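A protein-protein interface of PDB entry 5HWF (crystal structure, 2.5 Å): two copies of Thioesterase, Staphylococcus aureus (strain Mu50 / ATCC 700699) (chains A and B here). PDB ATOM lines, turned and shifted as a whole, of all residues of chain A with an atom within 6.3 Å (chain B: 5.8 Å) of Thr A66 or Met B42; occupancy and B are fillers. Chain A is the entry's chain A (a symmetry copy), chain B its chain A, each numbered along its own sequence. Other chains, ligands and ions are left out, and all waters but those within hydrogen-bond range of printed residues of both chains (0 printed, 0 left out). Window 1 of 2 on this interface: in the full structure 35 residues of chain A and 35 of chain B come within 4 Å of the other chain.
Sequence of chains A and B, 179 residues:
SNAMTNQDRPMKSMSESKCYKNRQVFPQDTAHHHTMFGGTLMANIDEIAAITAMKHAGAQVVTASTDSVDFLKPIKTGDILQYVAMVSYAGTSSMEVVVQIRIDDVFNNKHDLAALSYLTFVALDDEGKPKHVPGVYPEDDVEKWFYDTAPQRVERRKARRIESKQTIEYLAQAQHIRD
The backbone NH (N) of Thr B66 sits at hydrogen-bond distance from the backbone carbonyl oxygen (O) of Val A69 (2.9 Å). SD of Met B42 is in hydrogen-bond range of OG1 of Thr A66, 3.2 Å away. The side-chain sulfur (SD) of Met A42 sits at hydrogen-bond distance from the side-chain hydroxyl (OG1) of Thr B66, 3.2 Å away. The backbone NH (N) of Gly B39 sits at hydrogen-bond distance from the side-chain carboxylate (OD2) of Asp A46 (2.9 Å). The backbone carbonyl oxygen (O) of Val B69 is in hydrogen-bond range of the backbone NH (N) of Thr A66. The backbone NH (N) of Phe B71 sits at hydrogen-bond distance from the backbone carbonyl oxygen (O) of Ala A64 (3.2 Å). O of Asp B67 is in hydrogen-bond range of NH2 of Arg A160 (3.2 Å). OD2 of Asp B46 sits at hydrogen-bond distance from N of Gly A39. The backbone carbonyl oxygen of Asp A67 lies close to the backbone carbonyl oxygen of Asp B67 (2.9 Å).
Printed residues of chain A that touch a printed residue of chain B: Gly A38, Gly A39, Met A42, Ala A43, Asp A46, Thr A63, Ala A64, Ser A65, Thr A66, Asp A67, Ser A68, Val A69 and Arg A160. Hydrophobic or aromatic side chains of chain B within 4 Å of the printed part of chain A: Phe B37, Met B42, Ala B43, Val B69 and Phe B71. Along chain B the printed residues that touch a printed residue of chain A span positions 37 to 71. Among the printed residues, 24 pairs touch across the chains.
Gly A39 touches Ala B43, and with the chains exchanged Ala A43 touches Gly B39. Gly A39 touches Asp B46, and with the chains exchanged Asp A46 touches Gly B39. Met A42 touches Asp B46, and with the chains exchanged Asp A46 touches Met B42. Thr A66 touches Val B69, and with the chains exchanged Val A69 touches Thr B66. Of the 24 pairs that touch across the chains among the printed residues, 15 have their exchanged pair printed and touching as well.
Among the printed residues, pairs that only touch across the chains: Asp A46 with Phe B37, Ser A65 with Val B69, Ser A68 with Thr B66, Thr A66 with Ser B68, Thr A63 with Phe B71, Asp A46 with Gly B38, Gly A38 with Asp B46, Met A42 with Asp B46, Asp A46 with Met B42, Gly A39 with Ala B43, Ala A43 with Gly B39, Ser A65 with Phe B71, Arg A160 with Ser B68, Thr A66 with Phe B71 and Ser A65 with Asp B70.
Printed residues of chain B within 4 Å of Gly A38: Asp B46 (3.5 Å). Of the printed residues of chain B, Met A42 touches Asp B46 (3.5 Å) and Thr B66 (3.2 Å). Thr A66 touches four residues of chain B. Leu A119 touches none of the printed residues of chain B. Printed residues of chain A within 4 Å of Gly B39: Ala A43 (3.6 Å) and Asp A46 (2.9 Å). Met B42 touches just these residues of chain A: Asp A46 (3.5 Å) and Thr A66 (3.2 Å). Asn B44 touches none of the printed residues of chain A. The nearest residue of chain B that does not touch Thr A66 is Thr B66 (4.2 Å). The nearest printed residue of chain A that does not touch Ser B68 is Asp A67 (4.4 Å).
The backbone carbonyl oxygen (O) of Ser A68 sits at hydrogen-bond distance from the side-chain hydroxyl (OG) of Ser A117, 2.9 Å away. The backbone NH (N) of Thr A120 lies within hydrogen-bond range of the backbone carbonyl oxygen (O) of Ser A65 (2.9 Å). OD1 of Asp A67 sits at hydrogen-bond distance from OG of Ser A65 (2.6 Å). The backbone carbonyl oxygen (O) of Asp A67 is in hydrogen-bond range of the guanidinium group (NH2) of Arg A160 (3.4 Å). The side-chain carboxylate (OD1) of Asp A46 is in hydrogen-bond range of the side-chain hydroxyl (OG1) of Thr A63, at 2.6 Å. The backbone NH (N) of Ala A64 is in hydrogen-bond range of the backbone carbonyl oxygen (O) of Thr A120, at 2.9 Å.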
ATOM      1  N   GLY A  38     -13.811 -20.740   4.355  1.00  0.00           N
ATOM      2  CA  GLY A  38     -14.367 -21.863   5.098  1.00  0.00           C
ATOM      3  C   GLY A  38     -15.726 -21.580   5.704  1.00  0.00           C
ATOM      4  O   GLY A  38     -16.581 -22.473   5.726  1.00  0.00           O
ATOM      5  N   GLY A  39     -15.932 -20.345   6.177  1.00  0.00           N
ATOM      6  CA  GLY A  39     -17.202 -19.952   6.763  1.00  0.00           C
ATOM      7  C   GLY A  39     -18.353 -20.068   5.770  1.00  0.00           C
ATOM      8  O   GLY A  39     -19.473 -20.495   6.104  1.00  0.00           O
ATOM      9  N   MET A  42     -19.163 -23.610   5.230  1.00  0.00           N
ATOM     10  CA  MET A  42     -19.897 -24.110   6.388  1.00  0.00           C
ATOM     11  C   MET A  42     -21.364 -23.694   6.362  1.00  0.00           C
ATOM     12  O   MET A  42     -22.252 -24.478   6.719  1.00  0.00           O
ATOM     13  CB  MET A  42     -19.237 -23.641   7.679  1.00  0.00           C
ATOM     14  CG  MET A  42     -18.122 -24.562   8.144  1.00  0.00           C
ATOM     15  SD  MET A  42     -17.482 -24.099   9.760  1.00  0.00           S
ATOM     16  CE  MET A  42     -16.270 -22.858   9.302  1.00  0.00           C
ATOM     17  N   ALA A  43     -21.618 -22.464   5.931  1.00  0.00           N
ATOM     18  CA  ALA A  43     -22.984 -21.989   5.824  1.00  0.00           C
ATOM     19  C   ALA A  43     -23.770 -22.833   4.799  1.00  0.00           C
ATOM     20  O   ALA A  43     -24.906 -23.242   5.062  1.00  0.00           O
ATOM     21  CB  ALA A  43     -22.998 -20.503   5.467  1.00  0.00           C
ATOM     22  N   ILE A  45     -23.051 -25.985   3.751  1.00  0.00           N
ATOM     23  CA  ILE A  45     -23.158 -27.295   4.369  1.00  0.00           C
ATOM     24  C   ILE A  45     -24.369 -27.316   5.295  1.00  0.00           C
ATOM     25  O   ILE A  45     -25.224 -28.193   5.185  1.00  0.00           O
ATOM     26  CB  ILE A  45     -21.859 -27.659   5.134  1.00  0.00           C
ATOM     27  CG1 ILE A  45     -20.751 -27.990   4.126  1.00  0.00           C
ATOM     28  CG2 ILE A  45     -22.096 -28.815   6.125  1.00  0.00           C
ATOM     29  CD1 ILE A  45     -19.393 -28.103   4.746  1.00  0.00           C
ATOM     30  N   ASP A  46     -24.468 -26.319   6.173  1.00  0.00           N
ATOM     31  CA  ASP A  46     -25.591 -26.251   7.106  1.00  0.00           C
ATOM     32  C   ASP A  46     -26.938 -26.114   6.395  1.00  0.00           C
ATOM     33  O   ASP A  46     -27.938 -26.691   6.852  1.00  0.00           O
ATOM     34  CB  ASP A  46     -25.418 -25.084   8.083  1.00  0.00           C
ATOM     35  CG  ASP A  46     -26.366 -25.172   9.282  1.00  0.00           C
ATOM     36  OD1 ASP A  46     -26.446 -26.247   9.925  1.00  0.00           O
ATOM     37  OD2 ASP A  46     -27.054 -24.171   9.569  1.00  0.00           O
ATOM     38  N   THR A  63     -29.946 -26.806  13.898  1.00  0.00           N
ATOM     39  CA  THR A  63     -28.620 -27.365  14.115  1.00  0.00           C
ATOM     40  C   THR A  63     -28.274 -27.352  15.608  1.00  0.00           C
ATOM     41  O   THR A  63     -28.228 -26.296  16.229  1.00  0.00           O
ATOM     42  CB  THR A  63     -27.546 -26.604  13.348  1.00  0.00           C
ATOM     43  OG1 THR A  63     -28.020 -26.292  12.034  1.00  0.00           O
ATOM     44  CG2 THR A  63     -26.261 -27.435  13.274  1.00  0.00           C
ATOM     45  N   ALA A  64     -28.058 -28.540  16.168  1.00  0.00           N
ATOM     46  CA  ALA A  64     -27.697 -28.720  17.569  1.00  0.00           C
ATOM     47  C   ALA A  64     -26.190 -28.651  17.737  1.00  0.00           C
ATOM     48  O   ALA A  64     -25.678 -28.115  18.719  1.00  0.00           O
ATOM     49  CB  ALA A  64     -28.217 -30.045  18.088  1.00  0.00           C
ATOM     50  N   SER A  65     -25.480 -29.193  16.761  1.00  0.00           N
ATOM     51  CA  SER A  65     -24.041 -29.160  16.792  1.00  0.00           C
ATOM     52  C   SER A  65     -23.461 -29.462  15.430  1.00  0.00           C
ATOM     53  O   SER A  65     -24.064 -30.155  14.607  1.00  0.00           O
ATOM     54  CB  SER A  65     -23.491 -30.160  17.820  1.00  0.00           C
ATOM     55  OG  SER A  65     -23.683 -31.499  17.385  1.00  0.00           O
ATOM     56  N   THR A  66     -22.273 -28.932  15.209  1.00  0.00           N
ATOM     57  CA  THR A  66     -21.473 -29.327  14.076  1.00  0.00           C
ATOM     58  C   THR A  66     -20.428 -30.264  14.627  1.00  0.00           C
ATOM     59  O   THR A  66     -19.523 -29.851  15.337  1.00  0.00           O
ATOM     60  CB  THR A  66     -20.855 -28.116  13.378  1.00  0.00           C
ATOM     61  OG1 THR A  66     -21.915 -27.322  12.836  1.00  0.00           O
ATOM     62  CG2 THR A  66     -19.914 -28.544  12.257  1.00  0.00           C
ATOM     63  N   ASP A  67     -20.587 -31.546  14.333  1.00  0.00           N
ATOM     64  CA  ASP A  67     -19.719 -32.558  14.905  1.00  0.00           C
ATOM     65  C   ASP A  67     -18.358 -32.498  14.231  1.00  0.00           C
ATOM     66  O   ASP A  67     -17.342 -32.650  14.893  1.00  0.00           O
ATOM     67  CB  ASP A  67     -20.345 -33.938  14.770  1.00  0.00           C
ATOM     68  CG  ASP A  67     -21.801 -33.957  15.196  1.00  0.00           C
ATOM     69  OD1 ASP A  67     -22.143 -33.175  16.105  1.00  0.00           O
ATOM     70  OD2 ASP A  67     -22.599 -34.734  14.614  1.00  0.00           O
ATOM     71  N   SER A  68     -18.334 -32.270  12.919  1.00  0.00           N
ATOM     72  CA  SER A  68     -17.054 -32.021  12.251  1.00  0.00           C
ATOM     73  C   SER A  68     -17.208 -31.464  10.833  1.00  0.00           C
ATOM     74  O   SER A  68     -18.215 -31.676  10.153  1.00  0.00           O
ATOM     75  CB  SER A  68     -16.207 -33.301  12.190  1.00  0.00           C
ATOM     76  OG  SER A  68     -16.581 -34.123  11.087  1.00  0.00           O
ATOM     77  N   VAL A  69     -16.195 -30.728  10.405  1.00  0.00           N
ATOM     78  CA  VAL A  69     -16.036 -30.381   9.010  1.00  0.00           C
ATOM     79  C   VAL A  69     -14.573 -30.608   8.684  1.00  0.00           C
ATOM     80  O   VAL A  69     -13.710 -29.923   9.210  1.00  0.00           O
ATOM     81  CB  VAL A  69     -16.435 -28.910   8.696  1.00  0.00           C
ATOM     82  CG1 VAL A  69     -16.288 -28.628   7.210  1.00  0.00           C
ATOM     83  CG2 VAL A  69     -17.854 -28.619   9.148  1.00  0.00           C
ATOM     84  N   SER A 117     -18.566 -33.466   6.081  1.00  0.00           N
ATOM     85  CA  SER A 117     -19.085 -32.880   7.315  1.00  0.00           C
ATOM     86  C   SER A 117     -20.126 -33.750   8.026  1.00  0.00           C
ATOM     87  O   SER A 117     -20.975 -34.358   7.398  1.00  0.00           O
ATOM     88  CB  SER A 117     -19.694 -31.498   7.032  1.00  0.00           C
ATOM     89  OG  SER A 117     -20.164 -30.876   8.227  1.00  0.00           O
ATOM     90  N   TYR A 118     -20.057 -33.786   9.350  1.00  0.00           N
ATOM     91  CA  TYR A 118     -21.136 -34.351  10.139  1.00  0.00           C
ATOM     92  C   TYR A 118     -21.770 -33.278  11.018  1.00  0.00           C
ATOM     93  O   TYR A 118     -21.068 -32.502  11.687  1.00  0.00           O
ATOM     94  CB  TYR A 118     -20.627 -35.503  11.005  1.00  0.00           C
ATOM     95  CG  TYR A 118     -20.069 -36.663  10.223  1.00  0.00           C
ATOM     96  CD1 TYR A 118     -18.706 -36.799  10.050  1.00  0.00           C
ATOM     97  CD2 TYR A 118     -20.908 -37.628   9.658  1.00  0.00           C
ATOM     98  CE1 TYR A 118     -18.170 -37.855   9.353  1.00  0.00           C
ATOM     99  CE2 TYR A 118     -20.377 -38.704   8.944  1.00  0.00           C
ATOM    100  CZ  TYR A 118     -19.001 -38.803   8.803  1.00  0.00           C
ATOM    101  OH  TYR A 118     -18.433 -39.836   8.115  1.00  0.00           O
ATOM    102  N   LEU A 119     -23.101 -33.248  11.012  1.00  0.00           N
ATOM    103  CA  LEU A 119     -23.867 -32.330  11.842  1.00  0.00           C
ATOM    104  C   LEU A 119     -24.986 -33.081  12.530  1.00  0.00           C
ATOM    105  O   LEU A 119     -25.389 -34.159  12.092  1.00  0.00           O
ATOM    106  CB  LEU A 119     -24.470 -31.190  11.021  1.00  0.00           C
ATOM    107  CG  LEU A 119     -23.554 -30.402  10.099  1.00  0.00           C
ATOM    108  CD1 LEU A 119     -23.492 -31.115   8.748  1.00  0.00           C
ATOM    109  CD2 LEU A 119     -24.066 -28.994   9.960  1.00  0.00           C
ATOM    110  N   THR A 120     -25.495 -32.508  13.611  1.00  0.00           N
ATOM    111  CA  THR A 120     -26.591 -33.131  14.325  1.00  0.00           C
ATOM    112  C   THR A 120     -27.749 -32.154  14.368  1.00  0.00           C
ATOM    113  O   THR A 120     -27.587 -30.993  14.741  1.00  0.00           O
ATOM    114  CB  THR A 120     -26.169 -33.577  15.759  1.00  0.00           C
ATOM    115  OG1 THR A 120     -25.254 -34.683  15.674  1.00  0.00           O
ATOM    116  CG2 THR A 120     -27.372 -34.015  16.573  1.00  0.00           C
ATOM    117  N   ARG A 160     -17.657 -36.236  24.026  1.00  0.00           N
ATOM    118  CA  ARG A 160     -17.482 -34.816  23.807  1.00  0.00           C
ATOM    119  C   ARG A 160     -18.559 -33.990  24.492  1.00  0.00           C
ATOM    120  O   ARG A 160     -18.271 -32.930  24.974  1.00  0.00           O
ATOM    121  CB  ARG A 160     -17.364 -34.505  22.308  1.00  0.00           C
ATOM    122  CG  ARG A 160     -18.127 -33.294  21.774  1.00  0.00           C
ATOM    123  CD  ARG A 160     -17.297 -32.420  20.853  1.00  0.00           C
ATOM    124  NE  ARG A 160     -17.069 -33.083  19.580  1.00  0.00           N
ATOM    125  CZ  ARG A 160     -15.923 -33.080  18.917  1.00  0.00           C
ATOM    126  NH1 ARG A 160     -14.879 -32.428  19.395  1.00  0.00           N
ATOM    127  NH2 ARG A 160     -15.830 -33.741  17.778  1.00  0.00           N
ATOM    128  N   PHE B  37     -29.637 -18.268  12.020  1.00  0.00           N
ATOM    129  CA  PHE B  37     -29.343 -19.502  11.308  1.00  0.00           C
ATOM    130  C   PHE B  37     -27.929 -19.974  11.642  1.00  0.00           C
ATOM    131  O   PHE B  37     -26.981 -19.162  11.696  1.00  0.00           O
ATOM    132  CB  PHE B  37     -29.505 -19.300   9.798  1.00  0.00           C
ATOM    133  CG  PHE B  37     -29.230 -20.536   8.998  1.00  0.00           C
ATOM    134  CD1 PHE B  37     -29.969 -21.699   9.223  1.00  0.00           C
ATOM    135  CD2 PHE B  37     -28.235 -20.546   8.028  1.00  0.00           C
ATOM    136  CE1 PHE B  37     -29.726 -22.857   8.482  1.00  0.00           C
ATOM    137  CE2 PHE B  37     -27.976 -21.699   7.285  1.00  0.00           C
ATOM    138  CZ  PHE B  37     -28.732 -22.855   7.503  1.00  0.00           C
ATOM    139  N   GLY B  38     -27.788 -21.280  11.862  1.00  0.00           N
ATOM    140  CA  GLY B  38     -26.531 -21.872  12.301  1.00  0.00           C
ATOM    141  C   GLY B  38     -25.382 -21.642  11.342  1.00  0.00           C
ATOM    142  O   GLY B  38     -24.249 -21.428  11.789  1.00  0.00           O
ATOM    143  N   GLY B  39     -25.670 -21.668  10.036  1.00  0.00           N
ATOM    144  CA  GLY B  39     -24.653 -21.442   9.022  1.00  0.00           C
ATOM    145  C   GLY B  39     -24.020 -20.060   9.143  1.00  0.00           C
ATOM    146  O   GLY B  39     -22.800 -19.876   8.976  1.00  0.00           O
ATOM    147  N   THR B  40     -24.860 -19.076   9.446  1.00  0.00           N
ATOM    148  CA  THR B  40     -24.390 -17.705   9.619  1.00  0.00           C
ATOM    149  C   THR B  40     -23.454 -17.592  10.825  1.00  0.00           C
ATOM    150  O   THR B  40     -22.354 -17.004  10.748  1.00  0.00           O
ATOM    151  CB  THR B  40     -25.562 -16.742   9.805  1.00  0.00           C
ATOM    152  OG1 THR B  40     -26.528 -16.969   8.770  1.00  0.00           O
ATOM    153  CG2 THR B  40     -25.063 -15.297   9.768  1.00  0.00           C
ATOM    154  N   LEU B  41     -23.919 -18.155  11.935  1.00  0.00           N
ATOM    155  CA  LEU B  41     -23.118 -18.222  13.141  1.00  0.00           C
ATOM    156  C   LEU B  41     -21.774 -18.892  12.845  1.00  0.00           C
ATOM    157  O   LEU B  41     -20.732 -18.409  13.293  1.00  0.00           O
ATOM    158  CB  LEU B  41     -23.867 -18.965  14.246  1.00  0.00           C
ATOM    159  CG  LEU B  41     -23.078 -19.008  15.556  1.00  0.00           C
ATOM    160  CD1 LEU B  41     -22.643 -17.602  15.933  1.00  0.00           C
ATOM    161  CD2 LEU B  41     -23.916 -19.637  16.658  1.00  0.00           C
ATOM    162  N   MET B  42     -21.796 -19.973  12.065  1.00  0.00           N
ATOM    163  CA  MET B  42     -20.566 -20.688  11.746  1.00  0.00           C
ATOM    164  C   MET B  42     -19.614 -19.845  10.903  1.00  0.00           C
ATOM    165  O   MET B  42     -18.393 -19.874  11.106  1.00  0.00           O
ATOM    166  CB  MET B  42     -20.881 -21.999  11.035  1.00  0.00           C
ATOM    167  CG  MET B  42     -21.151 -23.145  11.995  1.00  0.00           C
ATOM    168  SD  MET B  42     -21.335 -24.720  11.146  1.00  0.00           S
ATOM    169  CE  MET B  42     -23.076 -24.669  10.713  1.00  0.00           C
ATOM    170  N   ALA B  43     -20.172 -19.090   9.965  1.00  0.00           N
ATOM    171  CA  ALA B  43     -19.356 -18.217   9.142  1.00  0.00           C
ATOM    172  C   ALA B  43     -18.663 -17.148  10.012  1.00  0.00           C
ATOM    173  O   ALA B  43     -17.464 -16.892   9.854  1.00  0.00           O
ATOM    174  CB  ALA B  43     -20.208 -17.587   8.040  1.00  0.00           C
ATOM    175  N   ASN B  44     -19.395 -16.563  10.959  1.00  0.00           N
ATOM    176  CA  ASN B  44     -18.784 -15.555  11.837  1.00  0.00           C
ATOM    177  C   ASN B  44     -17.718 -16.138  12.790  1.00  0.00           C
ATOM    178  O   ASN B  44     -16.640 -15.537  13.003  1.00  0.00           O
ATOM    179  CB  ASN B  44     -19.865 -14.836  12.639  1.00  0.00           C
ATOM    180  CG  ASN B  44     -20.581 -13.787  11.825  1.00  0.00           C
ATOM    181  OD1 ASN B  44     -20.020 -12.732  11.541  1.00  0.00           O
ATOM    182  ND2 ASN B  44     -21.828 -14.067  11.442  1.00  0.00           N
ATOM    183  N   ILE B  45     -18.026 -17.311  13.346  1.00  0.00           N
ATOM    184  CA  ILE B  45     -17.076 -18.062  14.149  1.00  0.00           C
ATOM    185  C   ILE B  45     -15.783 -18.241  13.361  1.00  0.00           C
ATOM    186  O   ILE B  45     -14.703 -17.913  13.850  1.00  0.00           O
ATOM    187  CB  ILE B  45     -17.666 -19.430  14.579  1.00  0.00           C
ATOM    188  CG1 ILE B  45     -18.730 -19.208  15.662  1.00  0.00           C
ATOM    189  CG2 ILE B  45     -16.562 -20.395  15.051  1.00  0.00           C
ATOM    190  CD1 ILE B  45     -19.542 -20.429  15.963  1.00  0.00           C
ATOM    191  N   ASP B  46     -15.900 -18.712  12.121  1.00  0.00           N
ATOM    192  CA  ASP B  46     -14.718 -18.921  11.285  1.00  0.00           C
ATOM    193  C   ASP B  46     -13.958 -17.623  11.007  1.00  0.00           C
ATOM    194  O   ASP B  46     -12.718 -17.634  10.956  1.00  0.00           O
ATOM    195  CB  ASP B  46     -15.102 -19.574   9.953  1.00  0.00           C
ATOM    196  CG  ASP B  46     -13.892 -20.127   9.197  1.00  0.00           C
ATOM    197  OD1 ASP B  46     -13.072 -20.861   9.801  1.00  0.00           O
ATOM    198  OD2 ASP B  46     -13.744 -19.808   8.000  1.00  0.00           O
ATOM    199  N   GLU B  47     -14.701 -16.526  10.802  1.00  0.00           N
ATOM    200  CA  GLU B  47     -14.098 -15.212  10.580  1.00  0.00           C
ATOM    201  C   GLU B  47     -13.203 -14.752  11.754  1.00  0.00           C
ATOM    202  O   GLU B  47     -12.018 -14.389  11.563  1.00  0.00           O
ATOM    203  CB  GLU B  47     -15.201 -14.169  10.305  1.00  0.00           C
ATOM    204  CG  GLU B  47     -15.809 -14.283   8.914  1.00  0.00           C
ATOM    205  CD  GLU B  47     -16.983 -13.341   8.672  1.00  0.00           C
ATOM    206  OE1 GLU B  47     -17.338 -12.554   9.575  1.00  0.00           O
ATOM    207  OE2 GLU B  47     -17.575 -13.411   7.571  1.00  0.00           O
ATOM    208  N   THR B  66     -13.243 -27.959  11.264  1.00  0.00           N
ATOM    209  CA  THR B  66     -14.072 -27.492  12.348  1.00  0.00           C
ATOM    210  C   THR B  66     -14.248 -28.678  13.261  1.00  0.00           C
ATOM    211  O   THR B  66     -14.931 -29.635  12.926  1.00  0.00           O
ATOM    212  CB  THR B  66     -15.406 -26.950  11.837  1.00  0.00           C
ATOM    213  OG1 THR B  66     -15.144 -25.795  11.034  1.00  0.00           O
ATOM    214  CG2 THR B  66     -16.328 -26.571  12.991  1.00  0.00           C
ATOM    215  N   ASP B  67     -13.584 -28.631  14.406  1.00  0.00           N
ATOM    216  CA  ASP B  67     -13.575 -29.763  15.313  1.00  0.00           C
ATOM    217  C   ASP B  67     -14.920 -29.862  16.014  1.00  0.00           C
ATOM    218  O   ASP B  67     -15.426 -30.957  16.211  1.00  0.00           O
ATOM    219  CB  ASP B  67     -12.435 -29.638  16.314  1.00  0.00           C
ATOM    220  CG  ASP B  67     -11.121 -29.274  15.651  1.00  0.00           C
ATOM    221  OD1 ASP B  67     -10.925 -29.698  14.494  1.00  0.00           O
ATOM    222  OD2 ASP B  67     -10.298 -28.557  16.274  1.00  0.00           O
ATOM    223  N   SER B  68     -15.503 -28.723  16.383  1.00  0.00           N
ATOM    224  CA  SER B  68     -16.875 -28.745  16.895  1.00  0.00           C
ATOM    225  C   SER B  68     -17.518 -27.357  16.971  1.00  0.00           C
ATOM    226  O   SER B  68     -16.844 -26.331  17.090  1.00  0.00           O
ATOM    227  CB  SER B  68     -16.934 -29.394  18.286  1.00  0.00           C
ATOM    228  OG  SER B  68     -16.606 -28.460  19.312  1.00  0.00           O
ATOM    229  N   VAL B  69     -18.838 -27.343  16.881  1.00  0.00           N
ATOM    230  CA  VAL B  69     -19.616 -26.174  17.232  1.00  0.00           C
ATOM    231  C   VAL B  69     -20.780 -26.679  18.062  1.00  0.00           C
ATOM    232  O   VAL B  69     -21.628 -27.402  17.562  1.00  0.00           O
ATOM    233  CB  VAL B  69     -20.139 -25.393  15.993  1.00  0.00           C
ATOM    234  CG1 VAL B  69     -20.907 -24.158  16.432  1.00  0.00           C
ATOM    235  CG2 VAL B  69     -18.998 -25.003  15.070  1.00  0.00           C
ATOM    236  N   ASP B  70     -20.808 -26.328  19.338  1.00  0.00           N
ATOM    237  CA  ASP B  70     -21.969 -26.611  20.150  1.00  0.00           C
ATOM    238  C   ASP B  70     -22.833 -25.356  20.235  1.00  0.00           C
ATOM    239  O   ASP B  70     -22.393 -24.294  20.712  1.00  0.00           O
ATOM    240  CB  ASP B  70     -21.559 -27.124  21.531  1.00  0.00           C
ATOM    241  CG  ASP B  70     -21.073 -28.576  21.492  1.00  0.00           C
ATOM    242  OD1 ASP B  70     -21.910 -29.487  21.280  1.00  0.00           O
ATOM    243  OD2 ASP B  70     -19.855 -28.812  21.666  1.00  0.00           O
ATOM    244  N   PHE B  71     -24.048 -25.493  19.699  1.00  0.00           N
ATOM    245  CA  PHE B  71     -25.105 -24.489  19.772  1.00  0.00           C
ATOM    246  C   PHE B  71     -25.916 -24.685  21.050  1.00  0.00           C
ATOM    247  O   PHE B  71     -26.799 -25.525  21.103  1.00  0.00           O
ATOM    248  CB  PHE B  71     -26.035 -24.570  18.541  1.00  0.00           C
ATOM    249  CG  PHE B  71     -25.318 -24.450  17.210  1.00  0.00           C
ATOM    250  CD1 PHE B  71     -24.851 -25.581  16.549  1.00  0.00           C
ATOM    251  CD2 PHE B  71     -25.112 -23.202  16.623  1.00  0.00           C
ATOM    252  CE1 PHE B  71     -24.189 -25.476  15.320  1.00  0.00           C
ATOM    253  CE2 PHE B  71     -24.449 -23.086  15.394  1.00  0.00           C
ATOM    254  CZ  PHE B  71     -23.991 -24.225  14.739  1.00  0.00           C
